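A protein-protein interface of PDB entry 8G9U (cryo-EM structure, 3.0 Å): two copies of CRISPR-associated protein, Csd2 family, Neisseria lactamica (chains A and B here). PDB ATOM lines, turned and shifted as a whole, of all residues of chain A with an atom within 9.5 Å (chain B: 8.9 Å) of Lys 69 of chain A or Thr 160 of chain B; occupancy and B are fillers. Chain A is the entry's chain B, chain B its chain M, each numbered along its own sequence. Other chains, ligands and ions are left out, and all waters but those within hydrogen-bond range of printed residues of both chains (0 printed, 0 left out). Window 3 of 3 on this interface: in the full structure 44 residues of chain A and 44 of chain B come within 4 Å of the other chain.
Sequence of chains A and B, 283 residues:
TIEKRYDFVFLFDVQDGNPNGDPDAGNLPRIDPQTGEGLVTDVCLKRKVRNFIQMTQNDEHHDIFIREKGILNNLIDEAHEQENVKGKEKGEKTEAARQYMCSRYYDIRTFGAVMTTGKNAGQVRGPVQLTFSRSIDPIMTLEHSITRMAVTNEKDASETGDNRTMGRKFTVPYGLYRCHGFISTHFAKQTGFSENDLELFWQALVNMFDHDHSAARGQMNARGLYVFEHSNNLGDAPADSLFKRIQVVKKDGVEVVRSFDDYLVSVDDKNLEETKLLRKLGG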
ATOM      1  N   ARG A  47     -17.530  -0.476  31.419  1.00  0.00           N
ATOM      2  CA  ARG A  47     -18.079  -1.665  32.054  1.00  0.00           C
ATOM      3  C   ARG A  47     -19.234  -1.314  32.960  1.00  0.00           C
ATOM      4  O   ARG A  47     -20.145  -2.113  33.150  1.00  0.00           O
ATOM      5  CB  ARG A  47     -17.015  -2.356  32.879  1.00  0.00           C
ATOM      6  CG  ARG A  47     -17.504  -3.557  33.657  1.00  0.00           C
ATOM      7  CD  ARG A  47     -17.634  -4.780  32.795  1.00  0.00           C
ATOM      8  NE  ARG A  47     -18.946  -5.020  32.232  1.00  0.00           N
ATOM      9  CZ  ARG A  47     -19.182  -5.987  31.360  1.00  0.00           C
ATOM     10  NH1 ARG A  47     -18.191  -6.759  30.964  1.00  0.00           N
ATOM     11  NH2 ARG A  47     -20.394  -6.180  30.879  1.00  0.00           N
ATOM     12  N   GLN A  54     -26.870  -4.430  31.254  1.00  0.00           N
ATOM     13  CA  GLN A  54     -27.242  -5.768  31.684  1.00  0.00           C
ATOM     14  C   GLN A  54     -28.312  -5.737  32.756  1.00  0.00           C
ATOM     15  O   GLN A  54     -28.992  -6.743  32.968  1.00  0.00           O
ATOM     16  CB  GLN A  54     -26.040  -6.532  32.224  1.00  0.00           C
ATOM     17  CG  GLN A  54     -25.033  -6.955  31.206  1.00  0.00           C
ATOM     18  CD  GLN A  54     -23.891  -7.708  31.842  1.00  0.00           C
ATOM     19  OE1 GLN A  54     -23.823  -7.828  33.063  1.00  0.00           O
ATOM     20  NE2 GLN A  54     -22.994  -8.233  31.021  1.00  0.00           N
ATOM     21  N   PHE A  65     -21.982  -8.400  25.379  1.00  0.00           N
ATOM     22  CA  PHE A  65     -20.638  -8.881  25.070  1.00  0.00           C
ATOM     23  C   PHE A  65     -19.920  -9.028  26.411  1.00  0.00           C
ATOM     24  O   PHE A  65     -19.056  -8.224  26.780  1.00  0.00           O
ATOM     25  CB  PHE A  65     -19.954  -7.933  24.083  1.00  0.00           C
ATOM     26  CG  PHE A  65     -19.009  -8.604  23.147  1.00  0.00           C
ATOM     27  CD1 PHE A  65     -19.475  -9.517  22.234  1.00  0.00           C
ATOM     28  CD2 PHE A  65     -17.662  -8.335  23.181  1.00  0.00           C
ATOM     29  CE1 PHE A  65     -18.627 -10.136  21.372  1.00  0.00           C
ATOM     30  CE2 PHE A  65     -16.808  -8.952  22.312  1.00  0.00           C
ATOM     31  CZ  PHE A  65     -17.292  -9.857  21.411  1.00  0.00           C
ATOM     32  N   ILE A  66     -20.272 -10.101  27.119  1.00  0.00           N
ATOM     33  CA  ILE A  66     -20.870 -10.117  28.453  1.00  0.00           C
ATOM     34  C   ILE A  66     -19.955 -10.544  29.586  1.00  0.00           C
ATOM     35  O   ILE A  66     -18.730 -10.585  29.457  1.00  0.00           O
ATOM     36  CB  ILE A  66     -22.108 -11.036  28.464  1.00  0.00           C
ATOM     37  CG1 ILE A  66     -21.722 -12.443  28.005  1.00  0.00           C
ATOM     38  CG2 ILE A  66     -23.229 -10.473  27.609  1.00  0.00           C
ATOM     39  CD1 ILE A  66     -22.855 -13.428  28.039  1.00  0.00           C
ATOM     40  N   ARG A  67     -20.594 -10.838  30.713  1.00  0.00           N
ATOM     41  CA  ARG A  67     -20.081 -11.062  32.055  1.00  0.00           C
ATOM     42  C   ARG A  67     -19.287 -12.366  32.106  1.00  0.00           C
ATOM     43  O   ARG A  67     -18.886 -12.892  31.067  1.00  0.00           O
ATOM     44  CB  ARG A  67     -21.295 -11.081  33.005  1.00  0.00           C
ATOM     45  CG  ARG A  67     -21.080 -11.319  34.491  1.00  0.00           C
ATOM     46  CD  ARG A  67     -20.323 -10.200  35.120  1.00  0.00           C
ATOM     47  NE  ARG A  67     -20.131 -10.407  36.552  1.00  0.00           N
ATOM     48  CZ  ARG A  67     -19.120 -11.097  37.068  1.00  0.00           C
ATOM     49  NH1 ARG A  67     -19.005 -11.242  38.380  1.00  0.00           N
ATOM     50  NH2 ARG A  67     -18.200 -11.616  36.268  1.00  0.00           N
ATOM     51  N   GLU A  68     -19.035 -12.871  33.307  1.00  0.00           N
ATOM     52  CA  GLU A  68     -18.110 -13.947  33.630  1.00  0.00           C
ATOM     53  C   GLU A  68     -18.007 -15.062  32.604  1.00  0.00           C
ATOM     54  O   GLU A  68     -16.995 -15.164  31.911  1.00  0.00           O
ATOM     55  CB  GLU A  68     -18.587 -14.545  34.950  1.00  0.00           C
ATOM     56  CG  GLU A  68     -17.780 -15.632  35.558  1.00  0.00           C
ATOM     57  CD  GLU A  68     -18.392 -16.044  36.870  1.00  0.00           C
ATOM     58  OE1 GLU A  68     -19.437 -15.463  37.226  1.00  0.00           O
ATOM     59  OE2 GLU A  68     -17.851 -16.933  37.551  1.00  0.00           O
ATOM     60  N   LYS A  69     -19.057 -15.860  32.434  1.00  0.00           N
ATOM     61  CA  LYS A  69     -19.005 -16.949  31.460  1.00  0.00           C
ATOM     62  C   LYS A  69     -19.183 -16.360  30.064  1.00  0.00           C
ATOM     63  O   LYS A  69     -20.104 -16.677  29.312  1.00  0.00           O
ATOM     64  CB  LYS A  69     -20.040 -18.021  31.768  1.00  0.00           C
ATOM     65  CG  LYS A  69     -19.757 -18.813  33.040  1.00  0.00           C
ATOM     66  CD  LYS A  69     -18.454 -19.614  32.957  1.00  0.00           C
ATOM     67  CE  LYS A  69     -17.390 -19.073  33.912  1.00  0.00           C
ATOM     68  NZ  LYS A  69     -16.210 -19.975  34.052  1.00  0.00           N
ATOM     69  N   GLY A  70     -18.248 -15.479  29.737  1.00  0.00           N
ATOM     70  CA  GLY A  70     -18.329 -14.648  28.568  1.00  0.00           C
ATOM     71  C   GLY A  70     -17.311 -15.024  27.528  1.00  0.00           C
ATOM     72  O   GLY A  70     -16.580 -14.151  27.064  1.00  0.00           O
ATOM     73  N   ILE A  71     -17.186 -16.307  27.199  1.00  0.00           N
ATOM     74  CA  ILE A  71     -16.273 -16.653  26.123  1.00  0.00           C
ATOM     75  C   ILE A  71     -16.743 -15.802  24.961  1.00  0.00           C
ATOM     76  O   ILE A  71     -17.837 -16.014  24.432  1.00  0.00           O
ATOM     77  CB  ILE A  71     -16.306 -18.146  25.758  1.00  0.00           C
ATOM     78  CG1 ILE A  71     -15.870 -19.028  26.922  1.00  0.00           C
ATOM     79  CG2 ILE A  71     -15.414 -18.412  24.577  1.00  0.00           C
ATOM     80  CD1 ILE A  71     -17.004 -19.437  27.825  1.00  0.00           C
ATOM     81  N   LEU A  72     -15.939 -14.819  24.568  1.00  0.00           N
ATOM     82  CA  LEU A  72     -16.436 -13.829  23.623  1.00  0.00           C
ATOM     83  C   LEU A  72     -16.651 -14.448  22.259  1.00  0.00           C
ATOM     84  O   LEU A  72     -17.546 -14.034  21.519  1.00  0.00           O
ATOM     85  CB  LEU A  72     -15.481 -12.648  23.528  1.00  0.00           C
ATOM     86  CG  LEU A  72     -15.429 -11.769  24.768  1.00  0.00           C
ATOM     87  CD1 LEU A  72     -14.570 -10.565  24.507  1.00  0.00           C
ATOM     88  CD2 LEU A  72     -16.815 -11.359  25.176  1.00  0.00           C
ATOM     89  N   ASN A  73     -15.850 -15.450  21.916  1.00  0.00           N
ATOM     90  CA  ASN A  73     -16.075 -16.145  20.661  1.00  0.00           C
ATOM     91  C   ASN A  73     -17.414 -16.861  20.664  1.00  0.00           C
ATOM     92  O   ASN A  73     -18.005 -17.069  19.608  1.00  0.00           O
ATOM     93  CB  ASN A  73     -14.947 -17.126  20.382  1.00  0.00           C
ATOM     94  CG  ASN A  73     -13.630 -16.443  20.208  1.00  0.00           C
ATOM     95  OD1 ASN A  73     -12.585 -17.080  20.223  1.00  0.00           O
ATOM     96  ND2 ASN A  73     -13.662 -15.132  20.064  1.00  0.00           N
ATOM     97  N   ASN A  74     -17.922 -17.232  21.834  1.00  0.00           N
ATOM     98  CA  ASN A  74     -19.234 -17.865  21.861  1.00  0.00           C
ATOM     99  C   ASN A  74     -20.318 -16.917  21.372  1.00  0.00           C
ATOM    100  O   ASN A  74     -21.400 -17.364  20.979  1.00  0.00           O
ATOM    101  CB  ASN A  74     -19.548 -18.367  23.262  1.00  0.00           C
ATOM    102  CG  ASN A  74     -18.745 -19.584  23.620  1.00  0.00           C
ATOM    103  OD1 ASN A  74     -17.803 -19.939  22.917  1.00  0.00           O
ATOM    104  ND2 ASN A  74     -19.108 -20.237  24.714  1.00  0.00           N
ATOM    105  N   LEU A  75     -20.052 -15.613  21.386  1.00  0.00           N
ATOM    106  CA  LEU A  75     -20.966 -14.632  20.822  1.00  0.00           C
ATOM    107  C   LEU A  75     -20.563 -14.246  19.408  1.00  0.00           C
ATOM    108  O   LEU A  75     -21.419 -14.086  18.528  1.00  0.00           O
ATOM    109  CB  LEU A  75     -21.002 -13.392  21.710  1.00  0.00           C
ATOM    110  CG  LEU A  75     -21.064 -13.710  23.201  1.00  0.00           C
ATOM    111  CD1 LEU A  75     -20.935 -12.453  24.022  1.00  0.00           C
ATOM    112  CD2 LEU A  75     -22.353 -14.425  23.525  1.00  0.00           C
ATOM    113  N   MET B 149     -13.982  -8.856  31.756  1.00  0.00           N
ATOM    114  CA  MET B 149     -14.768  -9.841  32.477  1.00  0.00           C
ATOM    115  C   MET B 149     -15.252 -10.925  31.544  1.00  0.00           C
ATOM    116  O   MET B 149     -16.412 -11.333  31.602  1.00  0.00           O
ATOM    117  CB  MET B 149     -15.935  -9.125  33.132  1.00  0.00           C
ATOM    118  CG  MET B 149     -15.465  -8.166  34.184  1.00  0.00           C
ATOM    119  SD  MET B 149     -16.778  -7.230  34.944  1.00  0.00           S
ATOM    120  CE  MET B 149     -17.549  -8.498  35.894  1.00  0.00           C
ATOM    121  N   ALA B 150     -14.360 -11.421  30.692  1.00  0.00           N
ATOM    122  CA  ALA B 150     -14.709 -12.365  29.645  1.00  0.00           C
ATOM    123  C   ALA B 150     -13.454 -12.794  28.911  1.00  0.00           C
ATOM    124  O   ALA B 150     -12.586 -11.960  28.669  1.00  0.00           O
ATOM    125  CB  ALA B 150     -15.694 -11.733  28.669  1.00  0.00           C
ATOM    126  N   VAL B 151     -13.343 -14.039  28.531  1.00  0.00           N
ATOM    127  CA  VAL B 151     -12.256 -14.447  27.652  1.00  0.00           C
ATOM    128  C   VAL B 151     -12.765 -14.415  26.229  1.00  0.00           C
ATOM    129  O   VAL B 151     -13.968 -14.500  25.978  1.00  0.00           O
ATOM    130  CB  VAL B 151     -11.714 -15.843  27.997  1.00  0.00           C
ATOM    131  CG1 VAL B 151     -11.146 -15.867  29.380  1.00  0.00           C
ATOM    132  CG2 VAL B 151     -12.806 -16.866  27.845  1.00  0.00           C
ATOM    133  N   GLU B 154     -11.593 -20.199  23.587  1.00  0.00           N
ATOM    134  CA  GLU B 154     -11.616 -21.276  24.566  1.00  0.00           C
ATOM    135  C   GLU B 154     -10.210 -21.329  25.148  1.00  0.00           C
ATOM    136  O   GLU B 154      -9.372 -22.161  24.792  1.00  0.00           O
ATOM    137  CB  GLU B 154     -12.035 -22.583  23.920  1.00  0.00           C
ATOM    138  CG  GLU B 154     -13.463 -22.558  23.426  1.00  0.00           C
ATOM    139  CD  GLU B 154     -14.461 -22.452  24.549  1.00  0.00           C
ATOM    140  OE1 GLU B 154     -14.180 -22.973  25.648  1.00  0.00           O
ATOM    141  OE2 GLU B 154     -15.532 -21.850  24.335  1.00  0.00           O
ATOM    142  N   LYS B 155      -9.955 -20.389  26.049  1.00  0.00           N
ATOM    143  CA  LYS B 155      -8.618 -20.081  26.513  1.00  0.00           C
ATOM    144  C   LYS B 155      -8.001 -21.283  27.216  1.00  0.00           C
ATOM    145  O   LYS B 155      -8.678 -22.251  27.566  1.00  0.00           O
ATOM    146  CB  LYS B 155      -8.664 -18.877  27.451  1.00  0.00           C
ATOM    147  CG  LYS B 155      -7.330 -18.221  27.710  1.00  0.00           C
ATOM    148  CD  LYS B 155      -6.673 -17.771  26.420  1.00  0.00           C
ATOM    149  CE  LYS B 155      -5.317 -17.152  26.698  1.00  0.00           C
ATOM    150  NZ  LYS B 155      -4.622 -16.780  25.444  1.00  0.00           N
ATOM    151  N   ASP B 156      -6.679 -21.222  27.390  1.00  0.00           N
ATOM    152  CA  ASP B 156      -6.005 -22.147  28.291  1.00  0.00           C
ATOM    153  C   ASP B 156      -6.700 -22.151  29.645  1.00  0.00           C
ATOM    154  O   ASP B 156      -7.222 -23.177  30.094  1.00  0.00           O
ATOM    155  CB  ASP B 156      -4.535 -21.750  28.440  1.00  0.00           C
ATOM    156  CG  ASP B 156      -3.754 -21.915  27.156  1.00  0.00           C
ATOM    157  OD1 ASP B 156      -4.121 -22.785  26.339  1.00  0.00           O
ATOM    158  OD2 ASP B 156      -2.766 -21.176  26.966  1.00  0.00           O
ATOM    159  N   ALA B 157      -6.711 -21.000  30.309  1.00  0.00           N
ATOM    160  CA  ALA B 157      -7.510 -20.808  31.515  1.00  0.00           C
ATOM    161  C   ALA B 157      -8.772 -19.996  31.218  1.00  0.00           C
ATOM    162  O   ALA B 157      -8.988 -18.913  31.763  1.00  0.00           O
ATOM    163  CB  ALA B 157      -6.670 -20.150  32.602  1.00  0.00           C
ATOM    164  N   SER B 158      -9.621 -20.534  30.342  1.00  0.00           N
ATOM    165  CA  SER B 158     -11.027 -20.131  30.306  1.00  0.00           C
ATOM    166  C   SER B 158     -11.814 -21.077  31.205  1.00  0.00           C
ATOM    167  O   SER B 158     -12.825 -21.664  30.831  1.00  0.00           O
ATOM    168  CB  SER B 158     -11.562 -20.145  28.884  1.00  0.00           C
ATOM    169  OG  SER B 158     -11.756 -21.470  28.438  1.00  0.00           O
ATOM    170  N   GLU B 159     -11.310 -21.205  32.418  1.00  0.00           N
ATOM    171  CA  GLU B 159     -11.535 -22.381  33.230  1.00  0.00           C
ATOM    172  C   GLU B 159     -12.819 -22.234  34.040  1.00  0.00           C
ATOM    173  O   GLU B 159     -13.635 -21.338  33.806  1.00  0.00           O
ATOM    174  CB  GLU B 159     -10.294 -22.619  34.101  1.00  0.00           C
ATOM    175  CG  GLU B 159     -10.165 -24.018  34.697  1.00  0.00           C
ATOM    176  CD  GLU B 159     -10.483 -25.115  33.706  1.00  0.00           C
ATOM    177  OE1 GLU B 159     -10.052 -25.017  32.537  1.00  0.00           O
ATOM    178  OE2 GLU B 159     -11.177 -26.075  34.094  1.00  0.00           O
ATOM    179  N   THR B 160     -13.005 -23.152  34.986  1.00  0.00           N
ATOM    180  CA  THR B 160     -14.179 -23.213  35.841  1.00  0.00           C
ATOM    181  C   THR B 160     -14.580 -21.863  36.409  1.00  0.00           C
ATOM    182  O   THR B 160     -15.659 -21.339  36.110  1.00  0.00           O
ATOM    183  CB  THR B 160     -13.879 -24.169  36.988  1.00  0.00           C
ATOM    184  OG1 THR B 160     -13.102 -23.474  37.967  1.00  0.00           O
ATOM    185  CG2 THR B 160     -13.071 -25.339  36.486  1.00  0.00           C
ATOM    186  N   GLY B 161     -13.693 -21.281  37.216  1.00  0.00           N
ATOM    187  CA  GLY B 161     -14.111 -20.232  38.133  1.00  0.00           C
ATOM    188  C   GLY B 161     -14.716 -19.028  37.441  1.00  0.00           C
ATOM    189  O   GLY B 161     -15.771 -18.533  37.839  1.00  0.00           O
ATOM    190  N   ASP B 162     -14.055 -18.544  36.396  1.00  0.00           N
ATOM    191  CA  ASP B 162     -14.501 -17.364  35.676  1.00  0.00           C
ATOM    192  C   ASP B 162     -13.622 -17.205  34.456  1.00  0.00           C
ATOM    193  O   ASP B 162     -12.486 -17.683  34.429  1.00  0.00           O
ATOM    194  CB  ASP B 162     -14.429 -16.105  36.548  1.00  0.00           C
ATOM    195  CG  ASP B 162     -13.077 -15.927  37.209  1.00  0.00           C
ATOM    196  OD1 ASP B 162     -12.204 -16.805  37.046  1.00  0.00           O
ATOM    197  OD2 ASP B 162     -12.889 -14.903  37.902  1.00  0.00           O
ATOM    198  N   ASN B 163     -14.157 -16.535  33.451  1.00  0.00           N
ATOM    199  CA  ASN B 163     -13.413 -16.215  32.246  1.00  0.00           C
ATOM    200  C   ASN B 163     -12.924 -14.786  32.378  1.00  0.00           C
ATOM    201  O   ASN B 163     -13.725 -13.849  32.406  1.00  0.00           O
ATOM    202  CB  ASN B 163     -14.289 -16.384  31.016  1.00  0.00           C
ATOM    203  CG  ASN B 163     -14.787 -17.780  30.865  1.00  0.00           C
ATOM    204  OD1 ASN B 163     -14.118 -18.733  31.242  1.00  0.00           O
ATOM    205  ND2 ASN B 163     -15.984 -17.918  30.334  1.00  0.00           N
ATOM    206  N   ARG B 164     -11.617 -14.620  32.485  1.00  0.00           N
ATOM    207  CA  ARG B 164     -11.009 -13.307  32.509  1.00  0.00           C
ATOM    208  C   ARG B 164      -9.843 -13.301  31.542  1.00  0.00           C
ATOM    209  O   ARG B 164      -9.202 -14.328  31.316  1.00  0.00           O
ATOM    210  CB  ARG B 164     -10.520 -12.939  33.890  1.00  0.00           C
ATOM    211  CG  ARG B 164     -11.337 -13.516  35.002  1.00  0.00           C
ATOM    212  CD  ARG B 164     -10.975 -12.859  36.290  1.00  0.00           C
ATOM    213  NE  ARG B 164     -11.415 -11.475  36.307  1.00  0.00           N
ATOM    214  CZ  ARG B 164     -12.642 -11.102  36.637  1.00  0.00           C
ATOM    215  NH1 ARG B 164     -13.535 -12.017  36.975  1.00  0.00           N
ATOM    216  NH2 ARG B 164     -12.976  -9.820  36.631  1.00  0.00           N
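The backbone carbonyl oxygen (O) of Met 149 of chain B is in hydrogen-bond range of the backbone NH (N) of Glu 68 of chain A, at 3.5 Å.
O of Gly 161 of chain B lies close to OE2 of Glu 68 of chain A (2.6 Å).
The side-chain amide nitrogen (ND2) of Asn 163 of chain B sits close to the backbone carbonyl oxygen (O) of Glu 68 of chain A, 3.3 Å away.
The backbone carbonyl oxygen (O) of Glu 159 of chain B sits at hydrogen-bond distance from the side-chain amino group (NZ) of Lys 69 of chain A, 2.9 Å away.
NZ of Lys 69 of chain A is in hydrogen-bond range of O of Thr 160 of chain B (2.5 Å).
The side-chain amide nitrogen (ND2) of Asn 163 of chain B sits close to the backbone NH (N) of Gly 70 of chain A.
N of Leu 72 of chain A is in hydrogen-bond range of O of Val 151 of chain B (2.4 Å).
The side-chain amide oxygen (OD1) of Asn 74 of chain A lies close to the side-chain carboxylate (OE2) of Glu 154 of chain B (3.3 Å).
The backbone carbonyl oxygen (O) of Ile 66 of chain A sits close to the backbone carbonyl oxygen (O) of Met 149 of chain B, at 3.2 Å.
The backbone carbonyl oxygen (O) of Met 149 of chain B lies close to the backbone carbonyl oxygen (O) of Arg 67 of chain A, 3.0 Å away.
The side-chain amino group (NZ) of Lys 69 of chain A lies close to the backbone NH (N) of Asp 162 of chain B, 3.5 Å away.
The backbone carbonyl oxygen of Gly 70 of chain A sits close to the backbone carbonyl oxygen of Val 151 of chain B (2.9 Å).
The guanidinium group (NH2) of Arg 47 of chain A lies close to the side-chain amide nitrogen (NE2) of Gln 54 of chain A (3.3 Å).
N of Ala 150 of chain B is in hydrogen-bond range of O of Asn 163 of chain B (3.0 Å).
O of Ser 158 of chain B lies close to OD1 of Asn 163 of chain B (3.2 Å).
OD2 of Asp 162 of chain B is in salt-bridge range of NH1 of Arg 164 of chain B (3.1 Å).
Among the printed residues, pairs that only touch across the chains: Arg 47 of chain A with Met 149 of chain B, Ile 66 of chain A with Ala 150 of chain B, Glu 68 of chain A with Asp 162 of chain B, Lys 69 of chain A with Gly 161 of chain B, Lys 69 of chain A with Asn 163 of chain B, Gly 70 of chain A with Ala 150 of chain B, Ile 71 of chain A with Val 151 of chain B, Ile 71 of chain A with Glu 154 of chain B, Ile 71 of chain A with Asn 163 of chain B and Leu 72 of chain A with Ala 150 of chain B.
Lys 69 of chain A touches just these residues of chain B: Glu 159, Thr 160, Gly 161, Asp 162 and Asn 163.
Of chain A, only Lys 69 comes within 4 Å of Thr 160 of chain B.
Of chain B, only Met 149 (3.5 Å), Gly 161 (2.6 Å), Asp 162 (3.5 Å) and Asn 163 (3.1 Å) come within 4 Å of Glu 68 of chain A.
Of chain A, only Lys 69 comes within 4 Å of Glu 159 of chain B.
Gly 161 of chain B touches just these residues of chain A: Glu 68 and Lys 69.
Printed residues of chain B within 4 Å of Ile 71 of chain A: Val 151, Glu 154 and Asn 163.
Printed residues of chain A within 4 Å of Ala 150 of chain B: Ile 66, Gly 70 and Leu 72.
Of the printed residues of chain A, Asp 162 of chain B touches Glu 68 (3.5 Å) and Lys 69 (3.5 Å).
Of the printed residues of chain B, Arg 47 of chain A touches Met 149 (3.4 Å).
Of the printed residues of chain B, Arg 67 of chain A touches Met 149.
Asp 156 of chain B touches none of the printed residues of chain A.
The nearest residue of chain B that does not touch Lys 69 of chain A is Ser 158 of chain B (5.0 Å).
The nearest printed residue of chain B that does not touch Arg 67 of chain A is Ala 150 of chain B (4.2 Å).
Hydrophobic or aromatic side chains of chain A within 4 Å of the printed part of chain B: Ile 71 and Leu 72.
Printed residues of chain B that touch a printed residue of chain A: Met 149, Ala 150, Val 151, Glu 154, Glu 159, Thr 160, Gly 161, Asp 162 and Asn 163.
Among the printed residues, no Asp or Glu carboxylate lies within 4 Å of a Lys or Arg side-chain nitrogen of the other chain.
No position is printed for both chains.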
